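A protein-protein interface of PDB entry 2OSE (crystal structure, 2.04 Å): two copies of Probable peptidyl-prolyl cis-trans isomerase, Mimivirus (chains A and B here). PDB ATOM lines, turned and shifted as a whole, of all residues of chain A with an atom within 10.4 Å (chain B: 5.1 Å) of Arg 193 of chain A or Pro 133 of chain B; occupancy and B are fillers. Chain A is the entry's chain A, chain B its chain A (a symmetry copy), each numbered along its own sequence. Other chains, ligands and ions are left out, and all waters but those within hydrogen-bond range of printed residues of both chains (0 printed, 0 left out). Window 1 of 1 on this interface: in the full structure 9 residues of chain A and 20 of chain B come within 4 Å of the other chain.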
ATOM      1  N   ASN A  24     -41.205  15.897   1.076  1.00  0.00           N
ATOM      2  CA  ASN A  24     -41.014  14.439   0.998  1.00  0.00           C
ATOM      3  C   ASN A  24     -42.125  13.648   1.661  1.00  0.00           C
ATOM      4  O   ASN A  24     -41.867  12.727   2.455  1.00  0.00           O
ATOM      5  CB  ASN A  24     -39.658  14.054   1.582  1.00  0.00           C
ATOM      6  CG  ASN A  24     -38.517  14.580   0.754  1.00  0.00           C
ATOM      7  OD1 ASN A  24     -38.604  14.630  -0.481  1.00  0.00           O
ATOM      8  ND2 ASN A  24     -37.438  14.987   1.421  1.00  0.00           N
ATOM      9  N   VAL A  84     -37.834  30.028  -4.949  1.00  0.00           N
ATOM     10  CA  VAL A  84     -37.423  30.111  -3.548  1.00  0.00           C
ATOM     11  C   VAL A  84     -36.071  30.779  -3.520  1.00  0.00           C
ATOM     12  O   VAL A  84     -35.215  30.526  -4.404  1.00  0.00           O
ATOM     13  CB  VAL A  84     -37.406  28.747  -2.800  1.00  0.00           C
ATOM     14  CG1 VAL A  84     -38.792  28.072  -2.829  1.00  0.00           C
ATOM     15  CG2 VAL A  84     -36.298  27.795  -3.337  1.00  0.00           C
ATOM     16  N   HIS A  86     -33.195  31.995  -0.598  1.00  0.00           N
ATOM     17  CA  HIS A  86     -32.643  32.076   0.776  1.00  0.00           C
ATOM     18  C   HIS A  86     -32.599  33.508   1.274  1.00  0.00           C
ATOM     19  O   HIS A  86     -32.164  34.430   0.549  1.00  0.00           O
ATOM     20  CB  HIS A  86     -31.250  31.386   0.839  1.00  0.00           C
ATOM     21  CG  HIS A  86     -30.591  31.423   2.189  1.00  0.00           C
ATOM     22  ND1 HIS A  86     -30.958  30.591   3.230  1.00  0.00           N
ATOM     23  CD2 HIS A  86     -29.528  32.132   2.638  1.00  0.00           C
ATOM     24  CE1 HIS A  86     -30.196  30.839   4.285  1.00  0.00           C
ATOM     25  NE2 HIS A  86     -29.312  31.760   3.947  1.00  0.00           N
ATOM     26  N   SER A 185     -33.507  27.714   6.362  1.00  0.00           N
ATOM     27  CA  SER A 185     -32.298  26.928   6.650  1.00  0.00           C
ATOM     28  C   SER A 185     -32.028  25.893   5.559  1.00  0.00           C
ATOM     29  O   SER A 185     -30.905  25.740   5.138  1.00  0.00           O
ATOM     30  CB  SER A 185     -32.396  26.231   7.991  1.00  0.00           C
ATOM     31  OG  SER A 185     -32.249  27.224   8.997  1.00  0.00           O
ATOM     32  N   MET A 186     -33.056  25.173   5.125  1.00  0.00           N
ATOM     33  CA  MET A 186     -32.864  24.114   4.142  1.00  0.00           C
ATOM     34  C   MET A 186     -32.513  24.604   2.746  1.00  0.00           C
ATOM     35  O   MET A 186     -32.068  23.802   1.917  1.00  0.00           O
ATOM     36  CB  MET A 186     -34.076  23.219   4.081  1.00  0.00           C
ATOM     37  CG  MET A 186     -34.254  22.449   5.350  1.00  0.00           C
ATOM     38  SD  MET A 186     -35.579  21.302   5.161  1.00  0.00           S
ATOM     39  CE  MET A 186     -36.927  22.308   5.709  1.00  0.00           C
ATOM     40  N   ILE A 187     -32.710  25.895   2.481  1.00  0.00           N
ATOM     41  CA  ILE A 187     -32.369  26.464   1.195  1.00  0.00           C
ATOM     42  C   ILE A 187     -31.091  27.315   1.207  1.00  0.00           C
ATOM     43  O   ILE A 187     -30.823  28.017   0.245  1.00  0.00           O
ATOM     44  CB  ILE A 187     -33.563  27.195   0.473  1.00  0.00           C
ATOM     45  CG1 ILE A 187     -33.988  28.479   1.203  1.00  0.00           C
ATOM     46  CG2 ILE A 187     -34.747  26.195   0.247  1.00  0.00           C
ATOM     47  CD1 ILE A 187     -35.168  29.235   0.496  1.00  0.00           C
ATOM     48  N   LYS A 188     -30.295  27.198   2.272  1.00  0.00           N
ATOM     49  CA  LYS A 188     -28.994  27.858   2.310  1.00  0.00           C
ATOM     50  C   LYS A 188     -28.191  27.408   1.075  1.00  0.00           C
ATOM     51  O   LYS A 188     -28.105  26.209   0.813  1.00  0.00           O
ATOM     52  CB  LYS A 188     -28.262  27.507   3.606  1.00  0.00           C
ATOM     53  CG  LYS A 188     -26.886  28.199   3.745  1.00  0.00           C
ATOM     54  CD  LYS A 188     -26.131  27.637   4.923  1.00  0.00           C
ATOM     55  CE  LYS A 188     -24.607  27.790   4.763  1.00  0.00           C
ATOM     56  NZ  LYS A 188     -24.168  29.232   4.735  1.00  0.00           N
ATOM     57  N   PRO A 189     -27.721  28.375   0.258  1.00  0.00           N
ATOM     58  CA  PRO A 189     -27.102  27.971  -1.016  1.00  0.00           C
ATOM     59  C   PRO A 189     -25.658  27.463  -0.919  1.00  0.00           C
ATOM     60  O   PRO A 189     -24.845  27.930  -0.095  1.00  0.00           O
ATOM     61  CB  PRO A 189     -27.176  29.234  -1.866  1.00  0.00           C
ATOM     62  CG  PRO A 189     -27.084  30.357  -0.859  1.00  0.00           C
ATOM     63  CD  PRO A 189     -27.840  29.847   0.373  1.00  0.00           C
ATOM     64  N   TYR A 190     -25.394  26.486  -1.773  1.00  0.00           N
ATOM     65  CA  TYR A 190     -24.098  25.854  -1.941  1.00  0.00           C
ATOM     66  C   TYR A 190     -24.053  25.524  -3.426  1.00  0.00           C
ATOM     67  O   TYR A 190     -25.029  25.003  -3.946  1.00  0.00           O
ATOM     68  CB  TYR A 190     -24.062  24.535  -1.175  1.00  0.00           C
ATOM     69  CG  TYR A 190     -23.867  24.679   0.304  1.00  0.00           C
ATOM     70  CD1 TYR A 190     -22.696  25.230   0.803  1.00  0.00           C
ATOM     71  CD2 TYR A 190     -24.846  24.255   1.208  1.00  0.00           C
ATOM     72  CE1 TYR A 190     -22.470  25.356   2.164  1.00  0.00           C
ATOM     73  CE2 TYR A 190     -24.628  24.367   2.616  1.00  0.00           C
ATOM     74  CZ  TYR A 190     -23.427  24.927   3.067  1.00  0.00           C
ATOM     75  OH  TYR A 190     -23.118  25.073   4.418  1.00  0.00           O
ATOM     76  N   ALA A 191     -22.948  25.842  -4.088  1.00  0.00           N
ATOM     77  CA  ALA A 191     -22.764  25.512  -5.511  1.00  0.00           C
ATOM     78  C   ALA A 191     -22.955  24.022  -5.722  1.00  0.00           C
ATOM     79  O   ALA A 191     -22.411  23.182  -4.946  1.00  0.00           O
ATOM     80  CB  ALA A 191     -21.401  25.968  -5.970  1.00  0.00           C
ATOM     81  N   GLY A 192     -23.826  23.694  -6.667  1.00  0.00           N
ATOM     82  CA  GLY A 192     -24.143  22.315  -7.028  1.00  0.00           C
ATOM     83  C   GLY A 192     -25.240  21.620  -6.249  1.00  0.00           C
ATOM     84  O   GLY A 192     -25.647  20.512  -6.604  1.00  0.00           O
ATOM     85  N   ARG A 193     -25.717  22.246  -5.171  1.00  0.00           N
ATOM     86  CA  ARG A 193     -26.751  21.661  -4.339  1.00  0.00           C
ATOM     87  C   ARG A 193     -28.112  22.097  -4.879  1.00  0.00           C
ATOM     88  O   ARG A 193     -28.422  23.293  -4.877  1.00  0.00           O
ATOM     89  CB  ARG A 193     -26.595  22.137  -2.881  1.00  0.00           C
ATOM     90  CG  ARG A 193     -27.770  21.788  -1.918  1.00  0.00           C
ATOM     91  CD  ARG A 193     -28.072  20.285  -1.822  1.00  0.00           C
ATOM     92  NE  ARG A 193     -26.930  19.490  -1.392  1.00  0.00           N
ATOM     93  CZ  ARG A 193     -26.925  18.164  -1.306  1.00  0.00           C
ATOM     94  NH1 ARG A 193     -28.001  17.482  -1.622  1.00  0.00           N
ATOM     95  NH2 ARG A 193     -25.829  17.516  -0.892  1.00  0.00           N
ATOM     96  N   LYS A 194     -28.937  21.154  -5.319  1.00  0.00           N
ATOM     97  CA  LYS A 194     -30.315  21.558  -5.597  1.00  0.00           C
ATOM     98  C   LYS A 194     -31.236  21.488  -4.363  1.00  0.00           C
ATOM     99  O   LYS A 194     -31.138  20.572  -3.524  1.00  0.00           O
ATOM    100  CB  LYS A 194     -30.916  20.920  -6.851  1.00  0.00           C
ATOM    101  CG  LYS A 194     -30.824  19.449  -6.962  1.00  0.00           C
ATOM    102  CD  LYS A 194     -31.207  19.039  -8.356  1.00  0.00           C
ATOM    103  CE  LYS A 194     -32.062  17.799  -8.322  1.00  0.00           C
ATOM    104  NZ  LYS A 194     -32.380  17.382  -9.708  1.00  0.00           N
ATOM    105  N   TYR A 195     -32.099  22.497  -4.268  1.00  0.00           N
ATOM    106  CA  TYR A 195     -32.983  22.678  -3.144  1.00  0.00           C
ATOM    107  C   TYR A 195     -33.977  21.522  -3.080  1.00  0.00           C
ATOM    108  O   TYR A 195     -34.333  20.930  -4.111  1.00  0.00           O
ATOM    109  CB  TYR A 195     -33.748  24.009  -3.265  1.00  0.00           C
ATOM    110  CG  TYR A 195     -32.913  25.277  -3.466  1.00  0.00           C
ATOM    111  CD1 TYR A 195     -31.874  25.615  -2.586  1.00  0.00           C
ATOM    112  CD2 TYR A 195     -33.189  26.147  -4.524  1.00  0.00           C
ATOM    113  CE1 TYR A 195     -31.100  26.797  -2.769  1.00  0.00           C
ATOM    114  CE2 TYR A 195     -32.444  27.322  -4.717  1.00  0.00           C
ATOM    115  CZ  TYR A 195     -31.397  27.641  -3.833  1.00  0.00           C
ATOM    116  OH  TYR A 195     -30.658  28.804  -4.033  1.00  0.00           O
ATOM    117  N   PRO A 196     -34.450  21.210  -1.862  1.00  0.00           N
ATOM    118  CA  PRO A 196     -35.583  20.300  -1.716  1.00  0.00           C
ATOM    119  C   PRO A 196     -36.861  20.924  -2.320  1.00  0.00           C
ATOM    120  O   PRO A 196     -36.910  22.128  -2.483  1.00  0.00           O
ATOM    121  CB  PRO A 196     -35.705  20.135  -0.190  1.00  0.00           C
ATOM    122  CG  PRO A 196     -35.035  21.348   0.393  1.00  0.00           C
ATOM    123  CD  PRO A 196     -33.940  21.698  -0.562  1.00  0.00           C
ATOM    124  N   THR A 197     -37.844  20.105  -2.698  1.00  0.00           N
ATOM    125  CA  THR A 197     -39.130  20.622  -3.216  1.00  0.00           C
ATOM    126  C   THR A 197     -40.214  20.691  -2.139  1.00  0.00           C
ATOM    127  O   THR A 197     -40.702  19.671  -1.650  1.00  0.00           O
ATOM    128  CB  THR A 197     -39.599  19.865  -4.465  1.00  0.00           C
ATOM    129  OG1 THR A 197     -38.691  20.160  -5.525  1.00  0.00           O
ATOM    130  CG2 THR A 197     -41.008  20.327  -4.911  1.00  0.00           C
ATOM    131  N   ASN B  83     -25.656  20.095 -12.419  1.00  0.00           N
ATOM    132  CA  ASN B  83     -25.208  21.465 -12.282  1.00  0.00           C
ATOM    133  C   ASN B  83     -23.833  21.430 -12.907  1.00  0.00           C
ATOM    134  O   ASN B  83     -22.992  20.576 -12.513  1.00  0.00           O
ATOM    135  CB  ASN B  83     -25.061  21.884 -10.798  1.00  0.00           C
ATOM    136  CG  ASN B  83     -26.367  22.355 -10.156  1.00  0.00           C
ATOM    137  OD1 ASN B  83     -26.505  23.533  -9.833  1.00  0.00           O
ATOM    138  ND2 ASN B  83     -27.317  21.441  -9.953  1.00  0.00           N
ATOM    139  N   ALA B 103     -31.026  12.592  -4.195  1.00  0.00           N
ATOM    140  CA  ALA B 103     -29.810  11.965  -3.700  1.00  0.00           C
ATOM    141  C   ALA B 103     -30.109  11.037  -2.520  1.00  0.00           C
ATOM    142  O   ALA B 103     -31.202  11.094  -1.917  1.00  0.00           O
ATOM    143  CB  ALA B 103     -28.794  13.034  -3.299  1.00  0.00           C
ATOM    144  N   LEU B 131     -17.446  16.471  -1.895  1.00  0.00           N
ATOM    145  CA  LEU B 131     -18.854  16.196  -1.591  1.00  0.00           C
ATOM    146  C   LEU B 131     -19.580  17.521  -1.325  1.00  0.00           C
ATOM    147  O   LEU B 131     -19.053  18.399  -0.681  1.00  0.00           O
ATOM    148  CB  LEU B 131     -19.019  15.233  -0.404  1.00  0.00           C
ATOM    149  CG  LEU B 131     -18.448  13.834  -0.614  1.00  0.00           C
ATOM    150  CD1 LEU B 131     -18.579  12.982   0.672  1.00  0.00           C
ATOM    151  CD2 LEU B 131     -19.077  13.111  -1.835  1.00  0.00           C
ATOM    152  N   VAL B 132     -20.791  17.644  -1.854  1.00  0.00           N
ATOM    153  CA  VAL B 132     -21.523  18.906  -1.760  1.00  0.00           C
ATOM    154  C   VAL B 132     -22.400  18.884  -0.485  1.00  0.00           C
ATOM    155  O   VAL B 132     -23.210  17.964  -0.303  1.00  0.00           O
ATOM    156  CB  VAL B 132     -22.358  19.139  -3.044  1.00  0.00           C
ATOM    157  CG1 VAL B 132     -23.193  20.450  -2.953  1.00  0.00           C
ATOM    158  CG2 VAL B 132     -21.428  19.161  -4.292  1.00  0.00           C
ATOM    159  N   PRO B 133     -22.213  19.875   0.404  1.00  0.00           N
ATOM    160  CA  PRO B 133     -22.995  19.890   1.639  1.00  0.00           C
ATOM    161  C   PRO B 133     -24.476  20.285   1.389  1.00  0.00           C
ATOM    162  O   PRO B 133     -24.826  20.842   0.338  1.00  0.00           O
ATOM    163  CB  PRO B 133     -22.295  20.955   2.489  1.00  0.00           C
ATOM    164  CG  PRO B 133     -21.653  21.862   1.506  1.00  0.00           C
ATOM    165  CD  PRO B 133     -21.300  21.031   0.303  1.00  0.00           C
ATOM    166  N   TYR B 134     -25.333  19.926   2.333  1.00  0.00           N
ATOM    167  CA  TYR B 134     -26.661  20.553   2.450  1.00  0.00           C
ATOM    168  C   TYR B 134     -26.962  20.861   3.938  1.00  0.00           C
ATOM    169  O   TYR B 134     -26.219  20.425   4.826  1.00  0.00           O
ATOM    170  CB  TYR B 134     -27.751  19.693   1.813  1.00  0.00           C
ATOM    171  CG  TYR B 134     -28.139  18.467   2.595  1.00  0.00           C
ATOM    172  CD1 TYR B 134     -29.194  18.519   3.521  1.00  0.00           C
ATOM    173  CD2 TYR B 134     -27.495  17.246   2.396  1.00  0.00           C
ATOM    174  CE1 TYR B 134     -29.593  17.407   4.223  1.00  0.00           C
ATOM    175  CE2 TYR B 134     -27.891  16.113   3.084  1.00  0.00           C
ATOM    176  CZ  TYR B 134     -28.938  16.204   4.005  1.00  0.00           C
ATOM    177  OH  TYR B 134     -29.333  15.106   4.700  1.00  0.00           O
ATOM    178  N   THR B 135     -28.013  21.653   4.176  1.00  0.00           N
ATOM    179  CA  THR B 135     -28.395  22.111   5.524  1.00  0.00           C
ATOM    180  C   THR B 135     -29.801  21.610   5.809  1.00  0.00           C
ATOM    181  O   THR B 135     -30.692  21.661   4.941  1.00  0.00           O
ATOM    182  CB  THR B 135     -28.295  23.639   5.634  1.00  0.00           C
ATOM    183  OG1 THR B 135     -26.951  24.047   5.368  1.00  0.00           O
ATOM    184  CG2 THR B 135     -28.631  24.120   7.031  1.00  0.00           C
ATOM    185  N   ARG B 141     -25.331  20.916   9.039  1.00  0.00           N
ATOM    186  CA  ARG B 141     -24.672  20.446   7.812  1.00  0.00           C
ATOM    187  C   ARG B 141     -24.610  18.918   7.684  1.00  0.00           C
ATOM    188  O   ARG B 141     -24.246  18.221   8.632  1.00  0.00           O
ATOM    189  CB  ARG B 141     -23.265  21.072   7.780  1.00  0.00           C
ATOM    190  CG  ARG B 141     -22.325  20.625   6.649  1.00  0.00           C
ATOM    191  CD  ARG B 141     -21.120  21.544   6.544  1.00  0.00           C
ATOM    192  NE  ARG B 141     -19.947  21.123   7.340  1.00  0.00           N
ATOM    193  CZ  ARG B 141     -19.481  21.748   8.435  1.00  0.00           C
ATOM    194  NH1 ARG B 141     -20.066  22.851   8.908  1.00  0.00           N
ATOM    195  NH2 ARG B 141     -18.407  21.276   9.065  1.00  0.00           N
ATOM    196  N   TYR B 142     -24.967  18.404   6.509  1.00  0.00           N
ATOM    197  CA  TYR B 142     -24.875  16.976   6.194  1.00  0.00           C
ATOM    198  C   TYR B 142     -24.402  16.778   4.749  1.00  0.00           C
ATOM    199  O   TYR B 142     -24.392  17.711   3.974  1.00  0.00           O
ATOM    200  CB  TYR B 142     -26.205  16.234   6.403  1.00  0.00           C
ATOM    201  CG  TYR B 142     -26.620  16.086   7.867  1.00  0.00           C
ATOM    202  CD1 TYR B 142     -26.055  15.086   8.700  1.00  0.00           C
ATOM    203  CD2 TYR B 142     -27.560  16.962   8.433  1.00  0.00           C
ATOM    204  CE1 TYR B 142     -26.436  14.969  10.062  1.00  0.00           C
ATOM    205  CE2 TYR B 142     -27.939  16.854   9.806  1.00  0.00           C
ATOM    206  CZ  TYR B 142     -27.373  15.867  10.597  1.00  0.00           C
ATOM    207  OH  TYR B 142     -27.768  15.772  11.917  1.00  0.00           O
ATOM    208  N   TYR B 143     -24.040  15.543   4.416  1.00  0.00           N
ATOM    209  CA  TYR B 143     -23.598  15.178   3.087  1.00  0.00           C
ATOM    210  C   TYR B 143     -24.387  13.993   2.622  1.00  0.00           C
ATOM    211  O   TYR B 143     -25.042  13.290   3.417  1.00  0.00           O
ATOM    212  CB  TYR B 143     -22.095  14.891   3.064  1.00  0.00           C
ATOM    213  CG  TYR B 143     -21.278  16.095   3.414  1.00  0.00           C
ATOM    214  CD1 TYR B 143     -20.781  16.934   2.421  1.00  0.00           C
ATOM    215  CD2 TYR B 143     -21.004  16.412   4.734  1.00  0.00           C
ATOM    216  CE1 TYR B 143     -20.044  18.035   2.737  1.00  0.00           C
ATOM    217  CE2 TYR B 143     -20.279  17.520   5.059  1.00  0.00           C
ATOM    218  CZ  TYR B 143     -19.808  18.340   4.062  1.00  0.00           C
ATOM    219  OH  TYR B 143     -19.044  19.440   4.372  1.00  0.00           O
ATOM    220  N   ASP B 144     -24.356  13.787   1.316  1.00  0.00           N
ATOM    221  CA  ASP B 144     -24.995  12.639   0.721  1.00  0.00           C
ATOM    222  C   ASP B 144     -24.164  12.177  -0.511  1.00  0.00           C
ATOM    223  O   ASP B 144     -22.938  12.403  -0.572  1.00  0.00           O
ATOM    224  CB  ASP B 144     -26.510  12.922   0.442  1.00  0.00           C
ATOM    225  CG  ASP B 144     -26.760  14.166  -0.427  1.00  0.00           C
ATOM    226  OD1 ASP B 144     -25.826  14.604  -1.169  1.00  0.00           O
ATOM    227  OD2 ASP B 144     -27.917  14.707  -0.381  1.00  0.00           O
ATOM    228  N   THR B 146     -24.254  13.431  -3.434  1.00  0.00           N
ATOM    229  CA  THR B 146     -23.957  14.605  -4.263  1.00  0.00           C
ATOM    230  C   THR B 146     -22.476  14.999  -4.256  1.00  0.00           C
ATOM    231  O   THR B 146     -21.894  15.275  -3.214  1.00  0.00           O
ATOM    232  CB  THR B 146     -24.786  15.859  -3.829  1.00  0.00           C
ATOM    233  OG1 THR B 146     -26.167  15.479  -3.674  1.00  0.00           O
ATOM    234  CG2 THR B 146     -24.673  16.982  -4.904  1.00  0.00           C
ATOM    235  N   ASP B 166     -16.827  23.986   3.290  1.00  0.00           N
ATOM    236  CA  ASP B 166     -17.642  22.796   3.465  1.00  0.00           C
ATOM    237  C   ASP B 166     -17.783  21.962   2.183  1.00  0.00           C
ATOM    238  O   ASP B 166     -18.362  20.885   2.220  1.00  0.00           O
ATOM    239  CB  ASP B 166     -19.052  23.157   3.948  1.00  0.00           C
ATOM    240  CG  ASP B 166     -19.081  23.723   5.365  1.00  0.00           C
ATOM    241  OD1 ASP B 166     -18.147  23.462   6.163  1.00  0.00           O
ATOM    242  OD2 ASP B 166     -20.084  24.419   5.669  1.00  0.00           O
ATOM    243  N   GLN B 167     -17.313  22.494   1.058  1.00  0.00           N
ATOM    244  CA  GLN B 167     -17.242  21.737  -0.192  1.00  0.00           C
ATOM    245  C   GLN B 167     -15.982  20.899  -0.073  1.00  0.00           C
ATOM    246  O   GLN B 167     -14.924  21.261  -0.590  1.00  0.00           O
ATOM    247  CB  GLN B 167     -17.220  22.683  -1.397  1.00  0.00           C
ATOM    248  CG  GLN B 167     -18.508  23.568  -1.530  1.00  0.00           C
ATOM    249  CD  GLN B 167     -19.588  22.997  -2.432  1.00  0.00           C
ATOM    250  OE1 GLN B 167     -19.630  21.803  -2.714  1.00  0.00           O
ATOM    251  NE2 GLN B 167     -20.471  23.878  -2.918  1.00  0.00           N
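The guanidinium group of Arg 193 of chain A is in salt-bridge range of the side-chain carboxylate of Asp 144 of chain B, 2.9 Å away.
The guanidinium group of Arg 193 of chain A sits at hydrogen-bond distance from the backbone carbonyl oxygen of Val 132 of chain B (2.7 Å).
OH of Tyr 190 of chain A sits at hydrogen-bond distance from OD2 of Asp 166 of chain B, at 3.3 Å.
The backbone carbonyl oxygen (O) of Ala 191 of chain A lies within hydrogen-bond range of the side-chain amide nitrogen (NE2) of Gln 167 of chain B (2.9 Å).
NH1 of Arg 193 of chain A lies within hydrogen-bond range of OG1 of Thr 146 of chain B (3.4 Å).
The guanidinium group (NE) of Arg 193 of chain A lies within hydrogen-bond range of the backbone carbonyl oxygen (O) of Pro 133 of chain B.
Hydrophobic or aromatic side chains of chain A that line the printed part of chain B: Met 186, Tyr 190 and Ala 191.
Of the 14 printed residues of chain B, 9 touch a printed residue of chain A.
Printed residues of chain B that touch a printed residue of chain A: Asn 83, Val 132, Pro 133, Tyr 134, Thr 135, Asp 144, Thr 146, Asp 166 and Gln 167.
Hydrophobic or aromatic side chains of chain B that line the printed part of chain A: Val 132, Pro 133 and Tyr 134.
Among the printed residues, 15 pairs touch across the chains.
Among the printed residues, Asp or Glu carboxylates within 4 Å of a Lys or Arg side-chain nitrogen of the other chain: Arg 193 of chain A with Asp 144 of chain B (2.9 Å).
No position is printed for both chains.
Of the 15 pairs that touch across the chains among the printed residues, none has its exchanged pair printed and touching as well.
The backbone carbonyl oxygen (O) of Thr 146 of chain B lies within hydrogen-bond range of the backbone NH (N) of Val 132 of chain B, 2.9 Å away.
N of Tyr 134 of chain B lies within hydrogen-bond range of O of Tyr 142 of chain B.
The side-chain hydroxyl (OH) of Tyr 143 of chain B lies within hydrogen-bond range of the backbone carbonyl oxygen (O) of Asp 166 of chain B (2.7 Å).
The guanidinium group (NE) of Arg 141 of chain B lies within salt-bridge range of the side-chain carboxylate (OD1) of Asp 166 of chain B, at 3.2 Å.
OG1 of Thr 146 of chain B sits at hydrogen-bond distance from OD1 of Asp 144 of chain B (2.7 Å).
Among the printed residues, merely in contact across the chains: Arg 193 of chain A with Tyr 134 of chain B (3.3 Å), Met 186 of chain A with Thr 135 of chain B (3.4 Å), Ser 185 of chain A with Thr 135 of chain B (3.4 Å), Ala 191 of chain A with Val 132 of chain B (3.5 Å), Tyr 190 of chain A with Pro 133 of chain B (3.5 Å), Tyr 190 of chain A with Thr 135 of chain B (3.6 Å), Lys 188 of chain A with Thr 135 of chain B (3.7 Å), Gly 192 of chain A with Asn 83 of chain B (3.8 Å) and Tyr 190 of chain A with Gln 167 of chain B (3.97 Å).
Arg 193 of chain A touches just these residues of chain B: Val 132 (2.7 Å), Pro 133 (3.0 Å), Tyr 134 (3.3 Å), Asp 144 (2.9 Å) and Thr 146 (3.4 Å).
Printed residues of chain A within 4 Å of Pro 133 of chain B: Tyr 190 (3.5 Å) and Arg 193 (3.0 Å).
Val 132 of chain B touches just these residues of chain A: Ala 191 and Arg 193.
No residue of chain A comes within 4 Å of Tyr 143 of chain B.
Of chain A, only Arg 193 (2.9 Å) comes within 4 Å of Asp 144 of chain B.
Of the printed residues of chain A, Thr 146 of chain B touches Arg 193.
Printed residues of chain A within 4 Å of Asp 166 of chain B: Tyr 190.
Printed residues of chain B within 4 Å of Lys 188 of chain A: Thr 135.
Printed residues of chain A within 4 Å of Asn 83 of chain B: Gly 192 (3.8 Å).
Val 84 of chain A touches none of the printed residues of chain B.
The nearest residue of chain A that does not touch Pro 133 of chain B is Ala 191 of chain A (5.8 Å).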
